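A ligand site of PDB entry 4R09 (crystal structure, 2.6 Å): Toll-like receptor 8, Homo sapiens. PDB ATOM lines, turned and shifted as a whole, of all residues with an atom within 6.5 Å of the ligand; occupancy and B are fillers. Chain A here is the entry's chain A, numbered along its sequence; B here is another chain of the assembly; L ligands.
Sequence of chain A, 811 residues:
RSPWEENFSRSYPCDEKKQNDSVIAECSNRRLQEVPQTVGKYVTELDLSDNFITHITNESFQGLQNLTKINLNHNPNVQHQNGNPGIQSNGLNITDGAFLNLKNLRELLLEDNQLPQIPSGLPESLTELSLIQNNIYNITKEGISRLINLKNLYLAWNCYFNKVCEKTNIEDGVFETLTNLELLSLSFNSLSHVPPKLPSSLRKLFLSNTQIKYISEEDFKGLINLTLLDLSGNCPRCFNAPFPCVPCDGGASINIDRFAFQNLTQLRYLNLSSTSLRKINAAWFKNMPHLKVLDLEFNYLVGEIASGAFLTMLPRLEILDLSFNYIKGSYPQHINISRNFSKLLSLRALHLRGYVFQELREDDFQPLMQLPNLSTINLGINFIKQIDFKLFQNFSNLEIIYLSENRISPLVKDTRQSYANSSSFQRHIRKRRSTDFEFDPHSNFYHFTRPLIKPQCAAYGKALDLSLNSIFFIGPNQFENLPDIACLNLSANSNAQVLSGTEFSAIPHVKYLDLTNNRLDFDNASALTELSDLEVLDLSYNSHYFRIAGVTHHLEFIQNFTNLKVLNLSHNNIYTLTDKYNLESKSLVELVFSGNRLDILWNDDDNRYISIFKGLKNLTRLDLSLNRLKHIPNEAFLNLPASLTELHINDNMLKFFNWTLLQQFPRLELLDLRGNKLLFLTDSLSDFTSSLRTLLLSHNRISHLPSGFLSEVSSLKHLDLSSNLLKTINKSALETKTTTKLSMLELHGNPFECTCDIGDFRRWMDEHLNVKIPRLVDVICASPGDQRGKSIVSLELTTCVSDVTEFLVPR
Residues that only touch the ligand: Val 498 (3.6 Å), Asp 523 (3.5 Å), Val 551 (3.4 Å), Tyr 326 of chain B (3.6 Å), Lys 328 of chain B (3.9 Å), Gly 329 of chain B (3.5 Å), Tyr 331 of chain B (3.5 Å), Val 356 of chain B (3.8 Å) and Phe 383 of chain B (3.5 Å). Of the 22 residues printed, 12 come within 4 Å of the ligand. The nearest printed residue that does not touch the ligand is Ser 330 of chain B (4.02 Å).
The side-chain carboxylate (OD1) of Asp 523 lies within hydrogen-bond range of the side-chain hydroxyl (OG1) of Thr 552 (2.5 Å). The guanidinium group of Arg 407 of chain B lies within hydrogen-bond range of the backbone carbonyl oxygen of Ala 496 (2.7 Å). The side-chain amide nitrogen (ND2) of Asn 240 of chain B sits at hydrogen-bond distance from the backbone carbonyl oxygen (O) of Val 551, at 2.9 Å. The backbone NH (N) of Asp 521 is in hydrogen-bond range of the backbone carbonyl oxygen (O) of Gln 497 (3.1 Å). The guanidinium group of Arg 407 of chain B lies within salt-bridge range of the side-chain carboxylate of Asp 521 (3.0 Å). The backbone NH of Val 356 of chain B is in hydrogen-bond range of the side-chain amide oxygen of Asn 382 of chain B (2.6 Å).
NH2 of Arg 407 of chain B sits at hydrogen-bond distance from O2 of the ligand (2.7 Å). A nitrogen (N2) of the ligand is in hydrogen-bond range of the side-chain carboxylate (OD2) of Asp 521, at 2.8 Å. The backbone NH (N) of Thr 552 lies within hydrogen-bond range of an oxygen (O6) of the ligand.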
ATOM      1  N   ALA A 496       3.936   2.377 -15.257  1.00  0.00           N
ATOM      2  CA  ALA A 496       3.149   2.627 -14.040  1.00  0.00           C
ATOM      3  C   ALA A 496       2.066   3.669 -14.203  1.00  0.00           C
ATOM      4  O   ALA A 496       1.476   4.095 -13.215  1.00  0.00           O
ATOM      5  CB  ALA A 496       4.079   3.040 -12.906  1.00  0.00           C
ATOM      6  N   GLN A 497       1.777   4.086 -15.438  1.00  0.00           N
ATOM      7  CA  GLN A 497       0.956   5.257 -15.636  1.00  0.00           C
ATOM      8  C   GLN A 497      -0.520   5.011 -15.442  1.00  0.00           C
ATOM      9  O   GLN A 497      -0.975   3.867 -15.454  1.00  0.00           O
ATOM     10  CB  GLN A 497       1.236   5.906 -17.002  1.00  0.00           C
ATOM     11  CG  GLN A 497       0.391   5.425 -18.136  1.00  0.00           C
ATOM     12  CD  GLN A 497       0.847   6.018 -19.465  1.00  0.00           C
ATOM     13  OE1 GLN A 497       1.303   5.296 -20.356  1.00  0.00           O
ATOM     14  NE2 GLN A 497       0.771   7.333 -19.590  1.00  0.00           N
ATOM     15  N   VAL A 498      -1.248   6.105 -15.223  1.00  0.00           N
ATOM     16  CA  VAL A 498      -2.707   6.109 -15.239  1.00  0.00           C
ATOM     17  C   VAL A 498      -3.156   6.405 -16.679  1.00  0.00           C
ATOM     18  O   VAL A 498      -2.987   7.525 -17.166  1.00  0.00           O
ATOM     19  CB  VAL A 498      -3.281   7.198 -14.274  1.00  0.00           C
ATOM     20  CG1 VAL A 498      -4.807   7.144 -14.238  1.00  0.00           C
ATOM     21  CG2 VAL A 498      -2.702   7.041 -12.862  1.00  0.00           C
ATOM     22  N   ASP A 521      -1.460   1.714 -13.257  1.00  0.00           N
ATOM     23  CA  ASP A 521      -2.286   2.258 -12.185  1.00  0.00           C
ATOM     24  C   ASP A 521      -3.649   2.547 -12.754  1.00  0.00           C
ATOM     25  O   ASP A 521      -3.821   3.492 -13.498  1.00  0.00           O
ATOM     26  CB  ASP A 521      -1.682   3.559 -11.632  1.00  0.00           C
ATOM     27  CG  ASP A 521      -2.357   4.039 -10.371  1.00  0.00           C
ATOM     28  OD1 ASP A 521      -3.211   3.295  -9.790  1.00  0.00           O
ATOM     29  OD2 ASP A 521      -2.039   5.165  -9.943  1.00  0.00           O
ATOM     30  N   ASP A 523      -6.549   3.990 -12.322  1.00  0.00           N
ATOM     31  CA  ASP A 523      -7.319   5.010 -11.658  1.00  0.00           C
ATOM     32  C   ASP A 523      -8.064   5.933 -12.648  1.00  0.00           C
ATOM     33  O   ASP A 523      -8.021   7.136 -12.482  1.00  0.00           O
ATOM     34  CB  ASP A 523      -6.347   5.834 -10.812  1.00  0.00           C
ATOM     35  CG  ASP A 523      -7.012   6.978 -10.132  1.00  0.00           C
ATOM     36  OD1 ASP A 523      -7.981   6.693  -9.356  1.00  0.00           O
ATOM     37  OD2 ASP A 523      -6.593   8.139 -10.403  1.00  0.00           O
ATOM     38  N   TYR A 545      -0.071  -2.473  -8.503  1.00  0.00           N
ATOM     39  CA  TYR A 545      -1.104  -1.728  -7.812  1.00  0.00           C
ATOM     40  C   TYR A 545      -2.242  -2.540  -7.253  1.00  0.00           C
ATOM     41  O   TYR A 545      -2.755  -2.237  -6.211  1.00  0.00           O
ATOM     42  CB  TYR A 545      -1.569  -0.531  -8.606  1.00  0.00           C
ATOM     43  CG  TYR A 545      -0.496   0.465  -8.743  1.00  0.00           C
ATOM     44  CD1 TYR A 545       0.187   0.589  -9.915  1.00  0.00           C
ATOM     45  CD2 TYR A 545      -0.120   1.243  -7.703  1.00  0.00           C
ATOM     46  CE1 TYR A 545       1.192   1.494 -10.057  1.00  0.00           C
ATOM     47  CE2 TYR A 545       0.886   2.146  -7.831  1.00  0.00           C
ATOM     48  CZ  TYR A 545       1.521   2.266  -9.015  1.00  0.00           C
ATOM     49  OH  TYR A 545       2.520   3.142  -9.155  1.00  0.00           O
ATOM     50  N   GLY A 550      -5.271   0.184  -0.644  1.00  0.00           N
ATOM     51  CA  GLY A 550      -5.749   1.545  -0.408  1.00  0.00           C
ATOM     52  C   GLY A 550      -5.676   2.496  -1.582  1.00  0.00           C
ATOM     53  O   GLY A 550      -6.050   3.672  -1.453  1.00  0.00           O
ATOM     54  N   VAL A 551      -5.131   2.040  -2.702  1.00  0.00           N
ATOM     55  CA  VAL A 551      -5.150   2.834  -3.877  1.00  0.00           C
ATOM     56  C   VAL A 551      -6.334   2.355  -4.695  1.00  0.00           C
ATOM     57  O   VAL A 551      -6.936   1.320  -4.380  1.00  0.00           O
ATOM     58  CB  VAL A 551      -3.845   2.749  -4.690  1.00  0.00           C
ATOM     59  CG1 VAL A 551      -2.719   3.456  -3.949  1.00  0.00           C
ATOM     60  CG2 VAL A 551      -3.477   1.316  -5.009  1.00  0.00           C
ATOM     61  N   THR A 552      -6.654   3.126  -5.737  1.00  0.00           N
ATOM     62  CA  THR A 552      -7.851   2.890  -6.540  1.00  0.00           C
ATOM     63  C   THR A 552      -7.567   1.842  -7.627  1.00  0.00           C
ATOM     64  O   THR A 552      -6.474   1.816  -8.218  1.00  0.00           O
ATOM     65  CB  THR A 552      -8.341   4.199  -7.177  1.00  0.00           C
ATOM     66  OG1 THR A 552      -7.278   4.819  -7.885  1.00  0.00           O
ATOM     67  CG2 THR A 552      -8.802   5.120  -6.135  1.00  0.00           C
ATOM     68  N   PHE B 239     -14.987   5.057   1.138  1.00  0.00           N
ATOM     69  CA  PHE B 239     -14.480   5.098  -0.238  1.00  0.00           C
ATOM     70  C   PHE B 239     -13.304   4.142  -0.443  1.00  0.00           C
ATOM     71  O   PHE B 239     -12.278   4.257   0.221  1.00  0.00           O
ATOM     72  CB  PHE B 239     -13.987   6.480  -0.608  1.00  0.00           C
ATOM     73  CG  PHE B 239     -13.444   6.557  -1.987  1.00  0.00           C
ATOM     74  CD1 PHE B 239     -14.223   6.153  -3.069  1.00  0.00           C
ATOM     75  CD2 PHE B 239     -12.159   6.947  -2.220  1.00  0.00           C
ATOM     76  CE1 PHE B 239     -13.730   6.212  -4.367  1.00  0.00           C
ATOM     77  CE2 PHE B 239     -11.643   7.011  -3.527  1.00  0.00           C
ATOM     78  CZ  PHE B 239     -12.437   6.656  -4.597  1.00  0.00           C
ATOM     79  N   ASN B 240     -13.444   3.253  -1.412  1.00  0.00           N
ATOM     80  CA  ASN B 240     -12.419   2.247  -1.700  1.00  0.00           C
ATOM     81  C   ASN B 240     -12.217   1.259  -0.547  1.00  0.00           C
ATOM     82  O   ASN B 240     -11.130   0.674  -0.397  1.00  0.00           O
ATOM     83  CB  ASN B 240     -11.102   2.924  -2.058  1.00  0.00           C
ATOM     84  CG  ASN B 240     -10.200   2.035  -2.846  1.00  0.00           C
ATOM     85  OD1 ASN B 240     -10.620   1.429  -3.816  1.00  0.00           O
ATOM     86  ND2 ASN B 240      -8.959   1.974  -2.465  1.00  0.00           N
ATOM     87  N   PHE B 324      -3.408   7.875   4.939  1.00  0.00           N
ATOM     88  CA  PHE B 324      -4.640   7.811   4.183  1.00  0.00           C
ATOM     89  C   PHE B 324      -5.706   8.819   4.635  1.00  0.00           C
ATOM     90  O   PHE B 324      -6.775   8.458   5.092  1.00  0.00           O
ATOM     91  CB  PHE B 324      -5.143   6.361   4.148  1.00  0.00           C
ATOM     92  CG  PHE B 324      -4.324   5.503   3.229  1.00  0.00           C
ATOM     93  CD1 PHE B 324      -4.440   5.642   1.855  1.00  0.00           C
ATOM     94  CD2 PHE B 324      -3.337   4.648   3.731  1.00  0.00           C
ATOM     95  CE1 PHE B 324      -3.634   4.907   0.992  1.00  0.00           C
ATOM     96  CE2 PHE B 324      -2.531   3.913   2.868  1.00  0.00           C
ATOM     97  CZ  PHE B 324      -2.689   4.038   1.495  1.00  0.00           C
ATOM     98  N   TYR B 326      -6.017  11.314   2.209  1.00  0.00           N
ATOM     99  CA  TYR B 326      -6.103  12.007   0.933  1.00  0.00           C
ATOM    100  C   TYR B 326      -7.573  12.355   0.699  1.00  0.00           C
ATOM    101  O   TYR B 326      -8.482  11.649   1.192  1.00  0.00           O
ATOM    102  CB  TYR B 326      -5.566  11.173  -0.251  1.00  0.00           C
ATOM    103  CG  TYR B 326      -6.362   9.911  -0.595  1.00  0.00           C
ATOM    104  CD1 TYR B 326      -5.949   8.669  -0.161  1.00  0.00           C
ATOM    105  CD2 TYR B 326      -7.504   9.970  -1.364  1.00  0.00           C
ATOM    106  CE1 TYR B 326      -6.638   7.527  -0.463  1.00  0.00           C
ATOM    107  CE2 TYR B 326      -8.197   8.809  -1.698  1.00  0.00           C
ATOM    108  CZ  TYR B 326      -7.745   7.597  -1.239  1.00  0.00           C
ATOM    109  OH  TYR B 326      -8.379   6.433  -1.514  1.00  0.00           O
ATOM    110  N   ILE B 327      -7.761  13.479   0.022  1.00  0.00           N
ATOM    111  CA  ILE B 327      -9.033  13.864  -0.550  1.00  0.00           C
ATOM    112  C   ILE B 327      -9.067  13.335  -1.962  1.00  0.00           C
ATOM    113  O   ILE B 327      -8.215  13.726  -2.777  1.00  0.00           O
ATOM    114  CB  ILE B 327      -9.136  15.407  -0.683  1.00  0.00           C
ATOM    115  CG1 ILE B 327      -9.121  16.088   0.669  1.00  0.00           C
ATOM    116  CG2 ILE B 327     -10.380  15.799  -1.481  1.00  0.00           C
ATOM    117  CD1 ILE B 327      -8.579  17.511   0.578  1.00  0.00           C
ATOM    118  N   LYS B 328     -10.025  12.485  -2.278  1.00  0.00           N
ATOM    119  CA  LYS B 328     -10.255  12.145  -3.683  1.00  0.00           C
ATOM    120  C   LYS B 328     -10.792  13.383  -4.352  1.00  0.00           C
ATOM    121  O   LYS B 328     -11.547  14.130  -3.724  1.00  0.00           O
ATOM    122  CB  LYS B 328     -11.252  11.004  -3.823  1.00  0.00           C
ATOM    123  CG  LYS B 328     -12.636  11.336  -3.343  1.00  0.00           C
ATOM    124  CD  LYS B 328     -13.593  10.159  -3.480  1.00  0.00           C
ATOM    125  CE  LYS B 328     -14.114   9.987  -4.894  1.00  0.00           C
ATOM    126  NZ  LYS B 328     -15.480   9.406  -4.874  1.00  0.00           N
ATOM    127  N   GLY B 329     -10.389  13.673  -5.587  1.00  0.00           N
ATOM    128  CA  GLY B 329      -9.252  13.092  -6.232  1.00  0.00           C
ATOM    129  C   GLY B 329      -8.266  14.215  -6.414  1.00  0.00           C
ATOM    130  O   GLY B 329      -7.820  14.496  -7.516  1.00  0.00           O
ATOM    131  N   SER B 330      -7.951  14.887  -5.311  1.00  0.00           N
ATOM    132  CA  SER B 330      -6.864  15.839  -5.292  1.00  0.00           C
ATOM    133  C   SER B 330      -5.580  15.102  -5.643  1.00  0.00           C
ATOM    134  O   SER B 330      -5.389  13.962  -5.260  1.00  0.00           O
ATOM    135  CB  SER B 330      -6.701  16.511  -3.920  1.00  0.00           C
ATOM    136  OG  SER B 330      -7.951  16.771  -3.301  1.00  0.00           O
ATOM    137  N   TYR B 331      -4.743  15.767  -6.421  1.00  0.00           N
ATOM    138  CA  TYR B 331      -3.372  15.346  -6.606  1.00  0.00           C
ATOM    139  C   TYR B 331      -2.563  16.615  -6.530  1.00  0.00           C
ATOM    140  O   TYR B 331      -1.924  17.035  -7.506  1.00  0.00           O
ATOM    141  CB  TYR B 331      -3.183  14.660  -7.950  1.00  0.00           C
ATOM    142  CG  TYR B 331      -1.874  13.926  -8.114  1.00  0.00           C
ATOM    143  CD1 TYR B 331      -1.238  13.289  -7.047  1.00  0.00           C
ATOM    144  CD2 TYR B 331      -1.283  13.815  -9.363  1.00  0.00           C
ATOM    145  CE1 TYR B 331      -0.044  12.605  -7.219  1.00  0.00           C
ATOM    146  CE2 TYR B 331      -0.095  13.128  -9.542  1.00  0.00           C
ATOM    147  CZ  TYR B 331       0.519  12.525  -8.466  1.00  0.00           C
ATOM    148  OH  TYR B 331       1.669  11.834  -8.678  1.00  0.00           O
ATOM    149  N   VAL B 356      -0.969  11.722  -0.804  1.00  0.00           N
ATOM    150  CA  VAL B 356      -1.015  11.822  -2.273  1.00  0.00           C
ATOM    151  C   VAL B 356      -0.775  13.248  -2.689  1.00  0.00           C
ATOM    152  O   VAL B 356      -1.649  14.076  -2.555  1.00  0.00           O
ATOM    153  CB  VAL B 356      -2.350  11.329  -2.862  1.00  0.00           C
ATOM    154  CG1 VAL B 356      -2.343  11.414  -4.376  1.00  0.00           C
ATOM    155  CG2 VAL B 356      -2.627   9.907  -2.412  1.00  0.00           C
ATOM    156  N   ASN B 382       2.426   7.764  -1.850  1.00  0.00           N
ATOM    157  CA  ASN B 382       1.959   9.121  -2.117  1.00  0.00           C
ATOM    158  C   ASN B 382       2.153   9.568  -3.574  1.00  0.00           C
ATOM    159  O   ASN B 382       2.118  10.735  -3.872  1.00  0.00           O
ATOM    160  CB  ASN B 382       2.674  10.123  -1.188  1.00  0.00           C
ATOM    161  CG  ASN B 382       2.119  10.115   0.222  1.00  0.00           C
ATOM    162  OD1 ASN B 382       0.981  10.498   0.427  1.00  0.00           O
ATOM    163  ND2 ASN B 382       2.914   9.669   1.190  1.00  0.00           N
ATOM    164  N   PHE B 383       2.319   8.629  -4.489  1.00  0.00           N
ATOM    165  CA  PHE B 383       2.373   8.966  -5.919  1.00  0.00           C
ATOM    166  C   PHE B 383       3.212  10.218  -6.161  1.00  0.00           C
ATOM    167  O   PHE B 383       2.961  10.968  -7.091  1.00  0.00           O
ATOM    168  CB  PHE B 383       0.963   9.107  -6.507  1.00  0.00           C
ATOM    169  CG  PHE B 383       0.171   7.808  -6.518  1.00  0.00           C
ATOM    170  CD1 PHE B 383       0.513   6.761  -7.379  1.00  0.00           C
ATOM    171  CD2 PHE B 383      -0.914   7.622  -5.667  1.00  0.00           C
ATOM    172  CE1 PHE B 383      -0.180   5.556  -7.373  1.00  0.00           C
ATOM    173  CE2 PHE B 383      -1.631   6.429  -5.671  1.00  0.00           C
ATOM    174  CZ  PHE B 383      -1.258   5.400  -6.524  1.00  0.00           C
ATOM    175  N   ARG B 407       6.427   7.756  -7.169  1.00  0.00           N
ATOM    176  CA  ARG B 407       6.673   7.869  -8.621  1.00  0.00           C
ATOM    177  C   ARG B 407       7.984   8.550  -8.876  1.00  0.00           C
ATOM    178  O   ARG B 407       8.150   9.202  -9.895  1.00  0.00           O
ATOM    179  CB  ARG B 407       5.570   8.642  -9.324  1.00  0.00           C
ATOM    180  CG  ARG B 407       4.175   8.008  -9.219  1.00  0.00           C
ATOM    181  CD  ARG B 407       3.318   8.459 -10.398  1.00  0.00           C
ATOM    182  NE  ARG B 407       2.007   7.807 -10.434  1.00  0.00           N
ATOM    183  CZ  ARG B 407       1.657   6.847 -11.282  1.00  0.00           C
ATOM    184  NH1 ARG B 407       2.544   6.365 -12.122  1.00  0.00           N
ATOM    185  NH2 ARG B 407       0.425   6.344 -11.273  1.00  0.00           N
HETATM  186  N1  LIG L   1      -3.789   9.166  -7.575  1.00  0.00           N
HETATM  187  C1  LIG L   1      -3.628   7.885  -8.090  1.00  0.00           C
HETATM  188  N2  LIG L   1      -2.574   7.750  -8.961  1.00  0.00           N
HETATM  189  C2  LIG L   1      -1.679   8.724  -9.346  1.00  0.00           C
HETATM  190  C3  LIG L   1      -1.897   9.999  -8.762  1.00  0.00           C
HETATM  191  C4  LIG L   1      -2.917  10.173  -7.908  1.00  0.00           C
HETATM  192  O1  LIG L   1      -4.376   6.949  -7.812  1.00  0.00           O
HETATM  193  O2  LIG L   1      -0.801   8.454 -10.178  1.00  0.00           O
HETATM  194  C5  LIG L   1      -4.850   9.412  -6.593  1.00  0.00           C
HETATM  195  C6  LIG L   1      -6.285   9.391  -7.132  1.00  0.00           C
HETATM  196  C7  LIG L   1      -7.064   8.582  -6.093  1.00  0.00           C
HETATM  197  C8  LIG L   1      -6.049   8.308  -4.965  1.00  0.00           C
HETATM  198  O3  LIG L   1      -6.798  10.715  -7.162  1.00  0.00           O
HETATM  199  O4  LIG L   1      -8.177   9.417  -5.694  1.00  0.00           O
HETATM  200  O5  LIG L   1      -4.761   8.452  -5.583  1.00  0.00           O
HETATM  201  C9  LIG L   1      -6.100   6.942  -4.322  1.00  0.00           C
HETATM  202  O6  LIG L   1      -5.334   5.989  -5.104  1.00  0.00           O
